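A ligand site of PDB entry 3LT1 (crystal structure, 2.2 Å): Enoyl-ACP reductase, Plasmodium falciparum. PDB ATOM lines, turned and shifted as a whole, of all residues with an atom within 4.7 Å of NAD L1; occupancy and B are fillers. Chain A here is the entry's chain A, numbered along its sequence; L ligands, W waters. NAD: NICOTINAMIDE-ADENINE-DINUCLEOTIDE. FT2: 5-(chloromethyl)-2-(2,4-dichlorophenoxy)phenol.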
ATOM      1  N   GLY A   9      -1.754   8.801  -2.106  1.00  0.00           N
ATOM      2  CA  GLY A   9      -2.464   7.767  -2.859  1.00  0.00           C
ATOM      3  C   GLY A   9      -3.966   7.741  -2.646  1.00  0.00           C
ATOM      4  O   GLY A   9      -4.512   6.721  -2.339  1.00  0.00           O
ATOM      5  N   ILE A  10      -4.629   8.890  -2.751  1.00  0.00           N
ATOM      6  CA  ILE A  10      -6.087   8.964  -2.727  1.00  0.00           C
ATOM      7  C   ILE A  10      -6.575   9.507  -4.062  1.00  0.00           C
ATOM      8  O   ILE A  10      -6.059  10.533  -4.547  1.00  0.00           O
ATOM      9  CB  ILE A  10      -6.588   9.819  -1.553  1.00  0.00           C
ATOM     10  CG1 ILE A  10      -6.528   8.979  -0.268  1.00  0.00           C
ATOM     11  CG2 ILE A  10      -8.043  10.269  -1.774  1.00  0.00           C
ATOM     12  CD1 ILE A  10      -6.735   9.731   1.015  1.00  0.00           C
ATOM     13  N   GLY A  11      -7.507   8.778  -4.684  1.00  0.00           N
ATOM     14  CA  GLY A  11      -8.101   9.155  -5.954  1.00  0.00           C
ATOM     15  C   GLY A  11      -9.623   9.264  -5.889  1.00  0.00           C
ATOM     16  O   GLY A  11     -10.229   9.877  -6.748  1.00  0.00           O
ATOM     17  N   ASP A  12     -10.225   8.653  -4.872  1.00  0.00           N
ATOM     18  CA  ASP A  12     -11.656   8.713  -4.659  1.00  0.00           C
ATOM     19  C   ASP A  12     -11.874   8.090  -3.299  1.00  0.00           C
ATOM     20  O   ASP A  12     -10.923   7.951  -2.517  1.00  0.00           O
ATOM     21  CB  ASP A  12     -12.356   7.866  -5.698  1.00  0.00           C
ATOM     22  CG  ASP A  12     -11.748   6.461  -5.790  1.00  0.00           C
ATOM     23  OD1 ASP A  12     -11.365   6.053  -6.889  1.00  0.00           O
ATOM     24  OD2 ASP A  12     -11.622   5.785  -4.766  1.00  0.00           O
ATOM     25  N   GLY A  15     -11.078   3.401  -2.035  1.00  0.00           N
ATOM     26  CA  GLY A  15      -9.831   2.665  -1.838  1.00  0.00           C
ATOM     27  C   GLY A  15      -9.439   2.631  -0.376  1.00  0.00           C
ATOM     28  O   GLY A  15     -10.171   3.119   0.460  1.00  0.00           O
ATOM     29  N   TYR A  16      -8.254   2.090  -0.092  1.00  0.00           N
ATOM     30  CA  TYR A  16      -7.769   2.011   1.289  1.00  0.00           C
ATOM     31  C   TYR A  16      -7.345   3.355   1.868  1.00  0.00           C
ATOM     32  O   TYR A  16      -7.426   3.558   3.084  1.00  0.00           O
ATOM     33  CB  TYR A  16      -6.613   1.004   1.401  1.00  0.00           C
ATOM     34  CG  TYR A  16      -7.119  -0.425   1.470  1.00  0.00           C
ATOM     35  CD1 TYR A  16      -8.091  -0.772   2.383  1.00  0.00           C
ATOM     36  CD2 TYR A  16      -6.629  -1.418   0.586  1.00  0.00           C
ATOM     37  CE1 TYR A  16      -8.570  -2.074   2.457  1.00  0.00           C
ATOM     38  CE2 TYR A  16      -7.078  -2.715   0.664  1.00  0.00           C
ATOM     39  CZ  TYR A  16      -8.055  -3.045   1.601  1.00  0.00           C
ATOM     40  OH  TYR A  16      -8.542  -4.313   1.733  1.00  0.00           O
ATOM     41  N   GLY A  17      -6.862   4.240   1.013  1.00  0.00           N
ATOM     42  CA  GLY A  17      -6.453   5.582   1.440  1.00  0.00           C
ATOM     43  C   GLY A  17      -7.566   6.316   2.174  1.00  0.00           C
ATOM     44  O   GLY A  17      -7.387   6.864   3.261  1.00  0.00           O
ATOM     45  N   TRP A  36      -2.667  11.898  -7.112  1.00  0.00           N
ATOM     46  CA  TRP A  36      -1.959  11.706  -8.371  1.00  0.00           C
ATOM     47  C   TRP A  36      -2.426  12.753  -9.413  1.00  0.00           C
ATOM     48  O   TRP A  36      -3.628  12.939  -9.613  1.00  0.00           O
ATOM     49  CB  TRP A  36      -2.213  10.281  -8.837  1.00  0.00           C
ATOM     50  CG  TRP A  36      -1.381   9.846  -9.976  1.00  0.00           C
ATOM     51  CD1 TRP A  36      -0.054  10.120 -10.212  1.00  0.00           C
ATOM     52  CD2 TRP A  36      -1.813   8.998 -11.045  1.00  0.00           C
ATOM     53  NE1 TRP A  36       0.351   9.523 -11.377  1.00  0.00           N
ATOM     54  CE2 TRP A  36      -0.710   8.816 -11.900  1.00  0.00           C
ATOM     55  CE3 TRP A  36      -3.034   8.402 -11.369  1.00  0.00           C
ATOM     56  CZ2 TRP A  36      -0.792   8.040 -13.055  1.00  0.00           C
ATOM     57  CZ3 TRP A  36      -3.124   7.632 -12.522  1.00  0.00           C
ATOM     58  CH2 TRP A  36      -2.008   7.455 -13.348  1.00  0.00           C
ATOM     59  N   VAL A  39      -5.564  12.677 -11.854  1.00  0.00           N
ATOM     60  CA  VAL A  39      -6.926  12.611 -11.288  1.00  0.00           C
ATOM     61  C   VAL A  39      -7.173  13.718 -10.261  1.00  0.00           C
ATOM     62  O   VAL A  39      -8.223  13.728  -9.604  1.00  0.00           O
ATOM     63  CB  VAL A  39      -7.272  11.219 -10.634  1.00  0.00           C
ATOM     64  CG1 VAL A  39      -6.874  10.059 -11.519  1.00  0.00           C
ATOM     65  CG2 VAL A  39      -6.639  11.052  -9.270  1.00  0.00           C
ATOM     66  N   PHE A  72       0.393  15.111  -6.185  1.00  0.00           N
ATOM     67  CA  PHE A  72       1.574  14.331  -5.756  1.00  0.00           C
ATOM     68  C   PHE A  72       1.827  13.211  -6.744  1.00  0.00           C
ATOM     69  O   PHE A  72       0.927  12.393  -7.009  1.00  0.00           O
ATOM     70  CB  PHE A  72       1.331  13.790  -4.340  1.00  0.00           C
ATOM     71  CG  PHE A  72       2.386  12.808  -3.865  1.00  0.00           C
ATOM     72  CD1 PHE A  72       3.550  13.260  -3.260  1.00  0.00           C
ATOM     73  CD2 PHE A  72       2.201  11.435  -4.012  1.00  0.00           C
ATOM     74  CE1 PHE A  72       4.538  12.334  -2.804  1.00  0.00           C
ATOM     75  CE2 PHE A  72       3.167  10.509  -3.581  1.00  0.00           C
ATOM     76  CZ  PHE A  72       4.334  10.971  -2.986  1.00  0.00           C
ATOM     77  N   ASP A  73       3.002  13.194  -7.352  1.00  0.00           N
ATOM     78  CA  ASP A  73       3.397  12.131  -8.258  1.00  0.00           C
ATOM     79  C   ASP A  73       4.656  11.414  -7.730  1.00  0.00           C
ATOM     80  O   ASP A  73       5.737  12.026  -7.627  1.00  0.00           O
ATOM     81  CB  ASP A  73       3.655  12.638  -9.671  1.00  0.00           C
ATOM     82  CG  ASP A  73       3.652  11.517 -10.705  1.00  0.00           C
ATOM     83  OD1 ASP A  73       4.071  10.382 -10.377  1.00  0.00           O
ATOM     84  OD2 ASP A  73       3.209  11.780 -11.851  1.00  0.00           O
ATOM     85  N   ALA A  74       4.505  10.129  -7.430  1.00  0.00           N
ATOM     86  CA  ALA A  74       5.572   9.355  -6.824  1.00  0.00           C
ATOM     87  C   ALA A  74       6.587   8.879  -7.860  1.00  0.00           C
ATOM     88  O   ALA A  74       7.572   8.259  -7.519  1.00  0.00           O
ATOM     89  CB  ALA A  74       4.986   8.161  -6.014  1.00  0.00           C
ATOM     90  N   SER A  75       6.309   9.165  -9.130  1.00  0.00           N
ATOM     91  CA  SER A  75       7.250   8.916 -10.218  1.00  0.00           C
ATOM     92  C   SER A  75       8.492   9.804 -10.132  1.00  0.00           C
ATOM     93  O   SER A  75       9.538   9.434 -10.656  1.00  0.00           O
ATOM     94  CB  SER A  75       6.602   9.143 -11.561  1.00  0.00           C
ATOM     95  OG  SER A  75       5.404   8.454 -11.661  1.00  0.00           O
ATOM     96  N   SER A 120      -0.028   4.672   0.200  1.00  0.00           N
ATOM     97  CA  SER A 120      -1.149   3.858  -0.202  1.00  0.00           C
ATOM     98  C   SER A 120      -1.312   3.952  -1.709  1.00  0.00           C
ATOM     99  O   SER A 120      -2.337   4.393  -2.213  1.00  0.00           O
ATOM    100  CB  SER A 120      -2.395   4.391   0.517  1.00  0.00           C
ATOM    101  OG  SER A 120      -3.484   3.544   0.279  1.00  0.00           O
ATOM    102  N   LEU A 121      -0.251   3.615  -2.443  1.00  0.00           N
ATOM    103  CA  LEU A 121      -0.255   3.753  -3.873  1.00  0.00           C
ATOM    104  C   LEU A 121       0.584   2.668  -4.506  1.00  0.00           C
ATOM    105  O   LEU A 121       1.548   2.157  -3.888  1.00  0.00           O
ATOM    106  CB  LEU A 121       0.274   5.147  -4.327  1.00  0.00           C
ATOM    107  CG  LEU A 121       1.740   5.484  -3.980  1.00  0.00           C
ATOM    108  CD1 LEU A 121       2.650   5.068  -5.148  1.00  0.00           C
ATOM    109  CD2 LEU A 121       1.911   7.005  -3.617  1.00  0.00           C
ATOM    110  N   ALA A 122       0.235   2.353  -5.753  1.00  0.00           N
ATOM    111  CA  ALA A 122       0.994   1.414  -6.589  1.00  0.00           C
ATOM    112  C   ALA A 122       0.653   1.692  -8.030  1.00  0.00           C
ATOM    113  O   ALA A 122      -0.389   2.269  -8.339  1.00  0.00           O
ATOM    114  CB  ALA A 122       0.662  -0.022  -6.213  1.00  0.00           C
ATOM    115  N   ASN A 123       1.521   1.266  -8.928  1.00  0.00           N
ATOM    116  CA  ASN A 123       1.256   1.387 -10.343  1.00  0.00           C
ATOM    117  C   ASN A 123       2.212   0.435 -11.056  1.00  0.00           C
ATOM    118  O   ASN A 123       3.304   0.109 -10.518  1.00  0.00           O
ATOM    119  CB  ASN A 123       1.451   2.832 -10.847  1.00  0.00           C
ATOM    120  CG  ASN A 123       0.431   3.198 -11.931  1.00  0.00           C
ATOM    121  OD1 ASN A 123       0.135   4.380 -12.142  1.00  0.00           O
ATOM    122  ND2 ASN A 123      -0.105   2.210 -12.602  1.00  0.00           N
ATOM    123  N   LYS A 145       7.449   2.867  -9.218  1.00  0.00           N
ATOM    124  CA  LYS A 145       6.258   3.503  -8.702  1.00  0.00           C
ATOM    125  C   LYS A 145       5.654   2.889  -7.455  1.00  0.00           C
ATOM    126  O   LYS A 145       5.072   3.625  -6.614  1.00  0.00           O
ATOM    127  CB  LYS A 145       5.279   3.546  -9.859  1.00  0.00           C
ATOM    128  CG  LYS A 145       5.810   4.674 -10.734  1.00  0.00           C
ATOM    129  CD  LYS A 145       5.297   4.618 -12.068  1.00  0.00           C
ATOM    130  CE  LYS A 145       5.995   5.675 -12.901  1.00  0.00           C
ATOM    131  NZ  LYS A 145       5.152   5.708 -14.086  1.00  0.00           N
ATOM    132  N   LEU A 170       1.067  -0.245   2.152  1.00  0.00           N
ATOM    133  CA  LEU A 170       0.156  -1.377   1.943  1.00  0.00           C
ATOM    134  C   LEU A 170       0.769  -2.397   0.993  1.00  0.00           C
ATOM    135  O   LEU A 170       1.368  -2.036  -0.006  1.00  0.00           O
ATOM    136  CB  LEU A 170      -1.200  -0.897   1.428  1.00  0.00           C
ATOM    137  CG  LEU A 170      -1.972   0.004   2.419  1.00  0.00           C
ATOM    138  CD1 LEU A 170      -3.082   0.724   1.685  1.00  0.00           C
ATOM    139  CD2 LEU A 170      -2.584  -0.761   3.538  1.00  0.00           C
ATOM    140  N   THR A 171       0.620  -3.658   1.326  1.00  0.00           N
ATOM    141  CA  THR A 171       1.136  -4.691   0.452  1.00  0.00           C
ATOM    142  C   THR A 171       0.074  -5.760   0.227  1.00  0.00           C
ATOM    143  O   THR A 171      -1.068  -5.631   0.702  1.00  0.00           O
ATOM    144  CB  THR A 171       2.519  -5.282   1.012  1.00  0.00           C
ATOM    145  OG1 THR A 171       3.096  -6.230   0.068  1.00  0.00           O
ATOM    146  CG2 THR A 171       2.297  -5.950   2.379  1.00  0.00           C
ATOM    147  N   TYR A 172       0.473  -6.819  -0.451  1.00  0.00           N
ATOM    148  CA  TYR A 172      -0.428  -7.896  -0.782  1.00  0.00           C
ATOM    149  C   TYR A 172       0.369  -9.215  -0.792  1.00  0.00           C
ATOM    150  O   TYR A 172       1.579  -9.247  -1.150  1.00  0.00           O
ATOM    151  CB  TYR A 172      -1.113  -7.595  -2.129  1.00  0.00           C
ATOM    152  CG  TYR A 172      -2.107  -8.663  -2.528  1.00  0.00           C
ATOM    153  CD1 TYR A 172      -3.190  -8.980  -1.707  1.00  0.00           C
ATOM    154  CD2 TYR A 172      -1.994  -9.336  -3.768  1.00  0.00           C
ATOM    155  CE1 TYR A 172      -4.109  -9.938  -2.074  1.00  0.00           C
ATOM    156  CE2 TYR A 172      -2.900 -10.315  -4.130  1.00  0.00           C
ATOM    157  CZ  TYR A 172      -3.961 -10.595  -3.280  1.00  0.00           C
ATOM    158  OH  TYR A 172      -4.865 -11.575  -3.632  1.00  0.00           O
ATOM    159  N   TYR A 182      -1.874 -11.513 -10.782  1.00  0.00           N
ATOM    160  CA  TYR A 182      -1.202 -10.323 -10.201  1.00  0.00           C
ATOM    161  C   TYR A 182       0.087 -10.103 -10.962  1.00  0.00           C
ATOM    162  O   TYR A 182       1.174 -10.391 -10.440  1.00  0.00           O
ATOM    163  CB  TYR A 182      -0.916 -10.502  -8.715  1.00  0.00           C
ATOM    164  CG  TYR A 182      -0.702  -9.247  -7.860  1.00  0.00           C
ATOM    165  CD1 TYR A 182      -1.740  -8.350  -7.619  1.00  0.00           C
ATOM    166  CD2 TYR A 182       0.536  -8.980  -7.292  1.00  0.00           C
ATOM    167  CE1 TYR A 182      -1.552  -7.218  -6.852  1.00  0.00           C
ATOM    168  CE2 TYR A 182       0.741  -7.871  -6.501  1.00  0.00           C
ATOM    169  CZ  TYR A 182      -0.295  -7.000  -6.273  1.00  0.00           C
ATOM    170  OH  TYR A 182      -0.061  -5.932  -5.462  1.00  0.00           O
ATOM    171  N   MET A 186       4.093  -6.542 -10.275  1.00  0.00           N
ATOM    172  CA  MET A 186       3.439  -6.120  -8.998  1.00  0.00           C
ATOM    173  C   MET A 186       3.782  -7.049  -7.818  1.00  0.00           C
ATOM    174  O   MET A 186       3.966  -6.598  -6.701  1.00  0.00           O
ATOM    175  CB  MET A 186       1.925  -5.973  -9.139  1.00  0.00           C
ATOM    176  CG  MET A 186       1.510  -4.644  -9.710  1.00  0.00           C
ATOM    177  SD  MET A 186       2.166  -3.168  -8.868  1.00  0.00           S
ATOM    178  CE  MET A 186       1.692  -3.460  -7.189  1.00  0.00           C
ATOM    179  N   LYS A 190       5.833  -5.790  -4.554  1.00  0.00           N
ATOM    180  CA  LYS A 190       5.382  -6.026  -3.187  1.00  0.00           C
ATOM    181  C   LYS A 190       6.409  -6.817  -2.365  1.00  0.00           C
ATOM    182  O   LYS A 190       6.551  -6.572  -1.173  1.00  0.00           O
ATOM    183  CB  LYS A 190       4.009  -6.731  -3.137  1.00  0.00           C
ATOM    184  CG  LYS A 190       2.830  -5.877  -3.674  1.00  0.00           C
ATOM    185  CD  LYS A 190       2.788  -4.471  -3.068  1.00  0.00           C
ATOM    186  CE  LYS A 190       1.431  -3.783  -3.417  1.00  0.00           C
ATOM    187  NZ  LYS A 190       1.340  -2.411  -2.885  1.00  0.00           N
ATOM    188  N   ALA A 217      -3.104  -6.176   3.150  1.00  0.00           N
ATOM    189  CA  ALA A 217      -4.585  -6.163   3.122  1.00  0.00           C
ATOM    190  C   ALA A 217      -5.186  -7.266   2.271  1.00  0.00           C
ATOM    191  O   ALA A 217      -4.588  -7.712   1.287  1.00  0.00           O
ATOM    192  CB  ALA A 217      -5.073  -4.838   2.644  1.00  0.00           C
ATOM    193  N   GLY A 218      -6.384  -7.699   2.654  1.00  0.00           N
ATOM    194  CA  GLY A 218      -7.186  -8.539   1.747  1.00  0.00           C
ATOM    195  C   GLY A 218      -7.861  -7.730   0.655  1.00  0.00           C
ATOM    196  O   GLY A 218      -7.681  -6.519   0.559  1.00  0.00           O
ATOM    197  N   PRO A 219      -8.686  -8.380  -0.185  1.00  0.00           N
ATOM    198  CA  PRO A 219      -9.200  -7.677  -1.404  1.00  0.00           C
ATOM    199  C   PRO A 219     -10.297  -6.642  -1.133  1.00  0.00           C
ATOM    200  O   PRO A 219     -11.190  -6.856  -0.301  1.00  0.00           O
ATOM    201  CB  PRO A 219      -9.729  -8.804  -2.255  1.00  0.00           C
ATOM    202  CG  PRO A 219     -10.197  -9.899  -1.186  1.00  0.00           C
ATOM    203  CD  PRO A 219      -9.240  -9.745  -0.014  1.00  0.00           C
ATOM    204  N   LEU A 220     -10.227  -5.529  -1.844  1.00  0.00           N
ATOM    205  CA  LEU A 220     -11.187  -4.431  -1.750  1.00  0.00           C
ATOM    206  C   LEU A 220     -11.428  -3.987  -3.161  1.00  0.00           C
ATOM    207  O   LEU A 220     -10.480  -3.866  -3.944  1.00  0.00           O
ATOM    208  CB  LEU A 220     -10.584  -3.251  -0.975  1.00  0.00           C
ATOM    209  CG  LEU A 220     -11.418  -1.975  -0.763  1.00  0.00           C
ATOM    210  CD1 LEU A 220     -12.586  -2.246   0.200  1.00  0.00           C
ATOM    211  CD2 LEU A 220     -10.509  -0.862  -0.222  1.00  0.00           C
ATOM    212  N   SER A 222     -11.521  -1.536  -5.216  1.00  0.00           N
ATOM    213  CA  SER A 222     -11.108  -0.163  -5.411  1.00  0.00           C
ATOM    214  C   SER A 222     -10.936   0.104  -6.918  1.00  0.00           C
ATOM    215  O   SER A 222     -10.982  -0.848  -7.716  1.00  0.00           O
ATOM    216  CB  SER A 222      -9.774   0.050  -4.708  1.00  0.00           C
ATOM    217  OG  SER A 222      -8.752  -0.666  -5.374  1.00  0.00           O
ATOM    218  N   ARG A 223     -10.688   1.367  -7.298  1.00  0.00           N
ATOM    219  CA  ARG A 223     -10.346   1.698  -8.699  1.00  0.00           C
ATOM    220  C   ARG A 223      -9.233   0.811  -9.230  1.00  0.00           C
ATOM    221  O   ARG A 223      -9.438   0.097 -10.201  1.00  0.00           O
ATOM    222  CB  ARG A 223      -9.976   3.192  -8.934  1.00  0.00           C
ATOM    223  CG  ARG A 223      -9.973   3.607 -10.464  1.00  0.00           C
ATOM    224  CD  ARG A 223      -8.623   3.458 -11.257  1.00  0.00           C
ATOM    225  NE  ARG A 223      -8.854   3.300 -12.708  1.00  0.00           N
ATOM    226  CZ  ARG A 223      -7.941   3.380 -13.693  1.00  0.00           C
ATOM    227  NH1 ARG A 223      -8.319   3.191 -14.952  1.00  0.00           N
ATOM    228  NH2 ARG A 223      -6.664   3.655 -13.437  1.00  0.00           N
ATOM    229  N   ALA A 224      -8.052   0.867  -8.616  1.00  0.00           N
ATOM    230  CA  ALA A 224      -6.931   0.063  -9.109  1.00  0.00           C
ATOM    231  C   ALA A 224      -7.230  -1.459  -9.208  1.00  0.00           C
ATOM    232  O   ALA A 224      -6.886  -2.108 -10.185  1.00  0.00           O
ATOM    233  CB  ALA A 224      -5.653   0.346  -8.301  1.00  0.00           C
ATOM    234  N   ALA A 225      -7.922  -2.010  -8.203  1.00  0.00           N
ATOM    235  CA  ALA A 225      -8.264  -3.422  -8.207  1.00  0.00           C
ATOM    236  C   ALA A 225      -8.980  -3.808  -9.498  1.00  0.00           C
ATOM    237  O   ALA A 225      -8.760  -4.895 -10.048  1.00  0.00           O
ATOM    238  CB  ALA A 225      -9.113  -3.755  -6.993  1.00  0.00           C
ATOM    239  N   ILE A 274     -10.752  -9.044  -9.242  1.00  0.00           N
ATOM    240  CA  ILE A 274     -11.101  -8.591  -7.909  1.00  0.00           C
ATOM    241  C   ILE A 274     -12.413  -9.193  -7.439  1.00  0.00           C
ATOM    242  O   ILE A 274     -12.599  -9.417  -6.246  1.00  0.00           O
ATOM    243  CB  ILE A 274     -11.130  -7.015  -7.768  1.00  0.00           C
ATOM    244  CG1 ILE A 274     -11.227  -6.589  -6.307  1.00  0.00           C
ATOM    245  CG2 ILE A 274     -12.321  -6.426  -8.545  1.00  0.00           C
ATOM    246  CD1 ILE A 274     -10.221  -7.154  -5.415  1.00  0.00           C
HETATM  247  PA  NAD L   1      -6.769   2.845  -5.221  1.00  0.00           P
HETATM  248  O1A NAD L   1      -6.833   3.054  -6.712  1.00  0.00           O
HETATM  249  O2A NAD L   1      -7.872   3.392  -4.331  1.00  0.00           O
HETATM  250  O5B NAD L   1      -5.364   3.419  -4.678  1.00  0.00           O
HETATM  251  C5B NAD L   1      -4.242   3.538  -5.539  1.00  0.00           C
HETATM  252  C4B NAD L   1      -3.921   5.022  -5.710  1.00  0.00           C
HETATM  253  O4B NAD L   1      -2.553   5.221  -6.078  1.00  0.00           O
HETATM  254  C3B NAD L   1      -4.758   5.687  -6.793  1.00  0.00           C
HETATM  255  O3B NAD L   1      -5.585   6.677  -6.194  1.00  0.00           O
HETATM  256  C2B NAD L   1      -3.767   6.345  -7.733  1.00  0.00           C
HETATM  257  O2B NAD L   1      -4.189   7.675  -8.062  1.00  0.00           O
HETATM  258  C1B NAD L   1      -2.478   6.368  -6.922  1.00  0.00           C
HETATM  259  N9A NAD L   1      -1.290   6.379  -7.812  1.00  0.00           N
HETATM  260  C8A NAD L   1      -1.044   5.586  -8.859  1.00  0.00           C
HETATM  261  N7A NAD L   1       0.157   5.918  -9.399  1.00  0.00           N
HETATM  262  C5A NAD L   1       0.648   6.941  -8.671  1.00  0.00           C
HETATM  263  C6A NAD L   1       1.890   7.756  -8.738  1.00  0.00           C
HETATM  264  N6A NAD L   1       2.830   7.530  -9.688  1.00  0.00           N
HETATM  265  N1A NAD L   1       2.059   8.732  -7.815  1.00  0.00           N
HETATM  266  C2A NAD L   1       1.116   8.945  -6.886  1.00  0.00           C
HETATM  267  N3A NAD L   1      -0.014   8.213  -6.810  1.00  0.00           N
HETATM  268  C4A NAD L   1      -0.265   7.223  -7.682  1.00  0.00           C
HETATM  269  O3  NAD L   1      -6.628   1.264  -4.944  1.00  0.00           O
HETATM  270  PN  NAD L   1      -6.233   0.697  -3.494  1.00  0.00           P
HETATM  271  O1N NAD L   1      -6.561  -0.773  -3.487  1.00  0.00           O
HETATM  272  O2N NAD L   1      -6.837   1.587  -2.434  1.00  0.00           O
HETATM  273  O5D NAD L   1      -4.629   0.845  -3.431  1.00  0.00           O
HETATM  274  C5D NAD L   1      -3.997   1.257  -2.219  1.00  0.00           C
HETATM  275  C4D NAD L   1      -2.865   0.311  -1.856  1.00  0.00           C
HETATM  276  O4D NAD L   1      -3.359  -0.876  -1.236  1.00  0.00           O
HETATM  277  C3D NAD L   1      -2.059  -0.124  -3.071  1.00  0.00           C
HETATM  278  O3D NAD L   1      -0.662   0.014  -2.777  1.00  0.00           O
HETATM  279  C2D NAD L   1      -2.396  -1.590  -3.248  1.00  0.00           C
HETATM  280  O2D NAD L   1      -1.255  -2.301  -3.759  1.00  0.00           O
HETATM  281  C1D NAD L   1      -2.738  -2.017  -1.836  1.00  0.00           C
HETATM  282  N1N NAD L   1      -3.617  -3.199  -1.809  1.00  0.00           N
HETATM  283  C2N NAD L   1      -4.837  -3.175  -2.363  1.00  0.00           C
HETATM  284  C3N NAD L   1      -5.675  -4.288  -2.320  1.00  0.00           C
HETATM  285  C7N NAD L   1      -7.048  -4.251  -2.946  1.00  0.00           C
HETATM  286  O7N NAD L   1      -7.693  -5.284  -3.020  1.00  0.00           O
HETATM  287  N7N NAD L   1      -7.519  -3.092  -3.404  1.00  0.00           N
HETATM  288  C4N NAD L   1      -5.230  -5.568  -1.649  1.00  0.00           C
HETATM  289  C5N NAD L   1      -3.889  -5.456  -1.093  1.00  0.00           C
HETATM  290  C6N NAD L   1      -3.151  -4.294  -1.198  1.00  0.00           C
HETATM  291  C1  FT2 L   2      -4.132  -3.869  -5.636  1.00  0.00           C
HETATM  292  C2  FT2 L   2      -3.260  -4.783  -5.096  1.00  0.00           C
HETATM  293  C3  FT2 L   2      -3.686  -6.065  -4.794  1.00  0.00           C
HETATM  294  C4  FT2 L   2      -4.982  -6.427  -5.075  1.00  0.00           C
HETATM  295  C5  FT2 L   2      -5.872  -5.513  -5.631  1.00  0.00           C
HETATM  296  C6  FT2 L   2      -5.459  -4.221  -5.918  1.00  0.00           C
HETATM  297  O7  FT2 L   2      -3.644  -2.615  -5.925  1.00  0.00           O
HETATM  298  C8  FT2 L   2      -3.071  -2.400  -7.150  1.00  0.00           C
HETATM  299  C9  FT2 L   2      -2.708  -1.118  -7.528  1.00  0.00           C
HETATM  300  C10 FT2 L   2      -2.153  -0.881  -8.777  1.00  0.00           C
HETATM  301  C11 FT2 L   2      -1.978  -1.961  -9.626  1.00  0.00           C
HETATM  302  C12 FT2 L   2      -2.330  -3.252  -9.272  1.00  0.00           C
HETATM  303  C13 FT2 L   2      -2.882  -3.480  -8.034  1.00  0.00           C
HETATM  304  C14 FT2 L   2      -5.382  -7.832  -4.740  1.00  0.00           C
HETATM  305 CL15 FT2 L   2      -7.091  -7.796  -4.289  1.00  0.00          CL
HETATM  306 CL16 FT2 L   2      -1.260  -1.619 -11.209  1.00  0.00          CL
HETATM  307 CL17 FT2 L   2      -2.954   0.305  -6.470  1.00  0.00          CL
HETATM  308  O18 FT2 L   2      -1.986  -4.435  -4.852  1.00  0.00           O
HETATM  309  O   HOH W   1      -5.973   3.695  -9.812  1.00  0.00           O
HETATM  310  O   HOH W   2      -8.343   5.612  -6.993  1.00  0.00           O
HETATM  311  O   HOH W   3      -7.871   6.313  -3.433  1.00  0.00           O
HETATM  312  O   HOH W   4      -4.347   9.576  -6.046  1.00  0.00           O
HETATM  313  O   HOH W   5      -5.794   4.280  -1.536  1.00  0.00           O
HETATM  314  O   HOH W   6     -10.502   3.358  -5.199  1.00  0.00           O
HETATM  315  O   HOH W   7       2.911   6.163 -12.443  1.00  0.00           O
HETATM  316  O   HOH W   8       1.301   1.094  -0.494  1.00  0.00           O
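The side-chain amide oxygen of Asn 123 lies close to a nitrogen (N7A) of NAD L1. The backbone carbonyl oxygen (O) of Leu 220 sits at hydrogen-bond distance from a nitrogen (N7N) of NAD L1, 3.1 Å away. The backbone NH (N) of Tyr 16 is in hydrogen-bond range of an oxygen (O2N) of NAD L1 (2.8 Å). N of Ala 74 lies within hydrogen-bond range of N1A of NAD L1, 2.8 Å away. The side-chain hydroxyl (OH) of Tyr 182 is in hydrogen-bond range of an oxygen (O18) of FT2 L2 (2.5 Å). The backbone carbonyl oxygen of Leu 121 lies within hydrogen-bond range of an oxygen (O3D) of NAD L1 (3.3 Å). The side-chain hydroxyl of Ser 222 sits at hydrogen-bond distance from an oxygen (O1N) of NAD L1. OD1 of Asp 73 lies within hydrogen-bond range of N6A of NAD L1, 3.2 Å away. An oxygen (O1A) of NAD L1 is in hydrogen-bond range of the backbone NH of Ala 224 (3.1 Å). N of Gly 11 is in hydrogen-bond range of O3B of NAD L1. An oxygen (O2D) of NAD L1 sits at hydrogen-bond distance from the side-chain amino group (NZ) of Lys 190 (2.7 Å). The side-chain hydroxyl of Ser 75 is in hydrogen-bond range of a nitrogen (N6A) of NAD L1 (3.4 Å). An oxygen (O7N) of NAD L1 lies within hydrogen-bond range of the backbone NH of Leu 220, 2.8 Å away.
O of Gly 9 touches C4B of NAD L1, at 3.8 Å. Ile 10 touches NAD L1. Gly 15 touches NAD L1. Trp 36 touches NAD L1 (CB to O2B, 3.4 Å). O of Phe 72 touches C2A of NAD L1, at 3.5 Å. OG of Ser 120 touches C5D of NAD L1, 3.4 Å away. Ala 122 touches NAD L1 (O to C8A, 3.4 Å). Leu 170 touches NAD L1 (CD1 to O4D, 3.3 Å). O of Thr 171 touches C6N of NAD L1 (3.1 Å). Tyr 172 touches NAD L1. Ala 217 touches NAD L1. O of Gly 218 touches C4N of NAD L1 (3.4 Å). Pro 219 touches NAD L1 (CA to O7N, 3.3 Å). Arg 223 touches NAD L1. Ala 225 touches NAD L1. Ile 274 touches NAD L1 (CD1 to O7N, 3.95 Å). Of the 33 residues printed, 27 come within 4 Å of NAD L1. The nearest printed residue that does not touch NAD L1 is Tyr 182 (4.2 Å).
O18 of FT2 L2 lies within hydrogen-bond range of O2D of NAD L1 (2.5 Å).
OH of Tyr 16 lies within hydrogen-bond range of O of Gly 218, 2.6 Å away. The side-chain carboxylate (OD1) of Asp 73 is in hydrogen-bond range of the side-chain hydroxyl (OG) of Ser 75, at 2.7 Å. O of Leu 170 sits at hydrogen-bond distance from NZ of Lys 190 (2.9 Å). The side-chain hydroxyl (OG) of Ser 222 is in hydrogen-bond range of the backbone NH (N) of Ala 225, at 3.2 Å. The backbone carbonyl oxygen of Thr 171 sits at hydrogen-bond distance from the backbone NH of Ala 217.
Water W6 lies within hydrogen-bond range of the side-chain carboxylate of Asp 12 (2.7 Å), an oxygen (O2A) of NAD L1 (2.8 Å), the backbone NH of Arg 223 (2.9 Å) and the backbone NH of Gly 15 (3.2 Å). Water W4 lies within hydrogen-bond range of O of Ile 10 (2.5 Å), O2B of NAD L1 (2.8 Å) and N of Trp 36 (3.1 Å). Water W2 lies within hydrogen-bond range of O1A of NAD L1 (3.0 Å) and OD1 of Asp 12 (3.1 Å). Water W3 bridges the backbone NH (N) of Gly 11 (2.8 Å) and an oxygen (O2A) of NAD L1 (3.1 Å). Water W7 lies within hydrogen-bond range of the side-chain amino group (NZ) of Lys 145 (2.8 Å), a nitrogen (N6A) of NAD L1 (3.1 Å), the side-chain amide oxygen (OD1) of Asn 123 (3.3 Å) and the side-chain hydroxyl (OG) of Ser 75 (3.5 Å). Water W8 bridges the backbone NH (N) of Leu 170 and an oxygen (O3D) of NAD L1.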
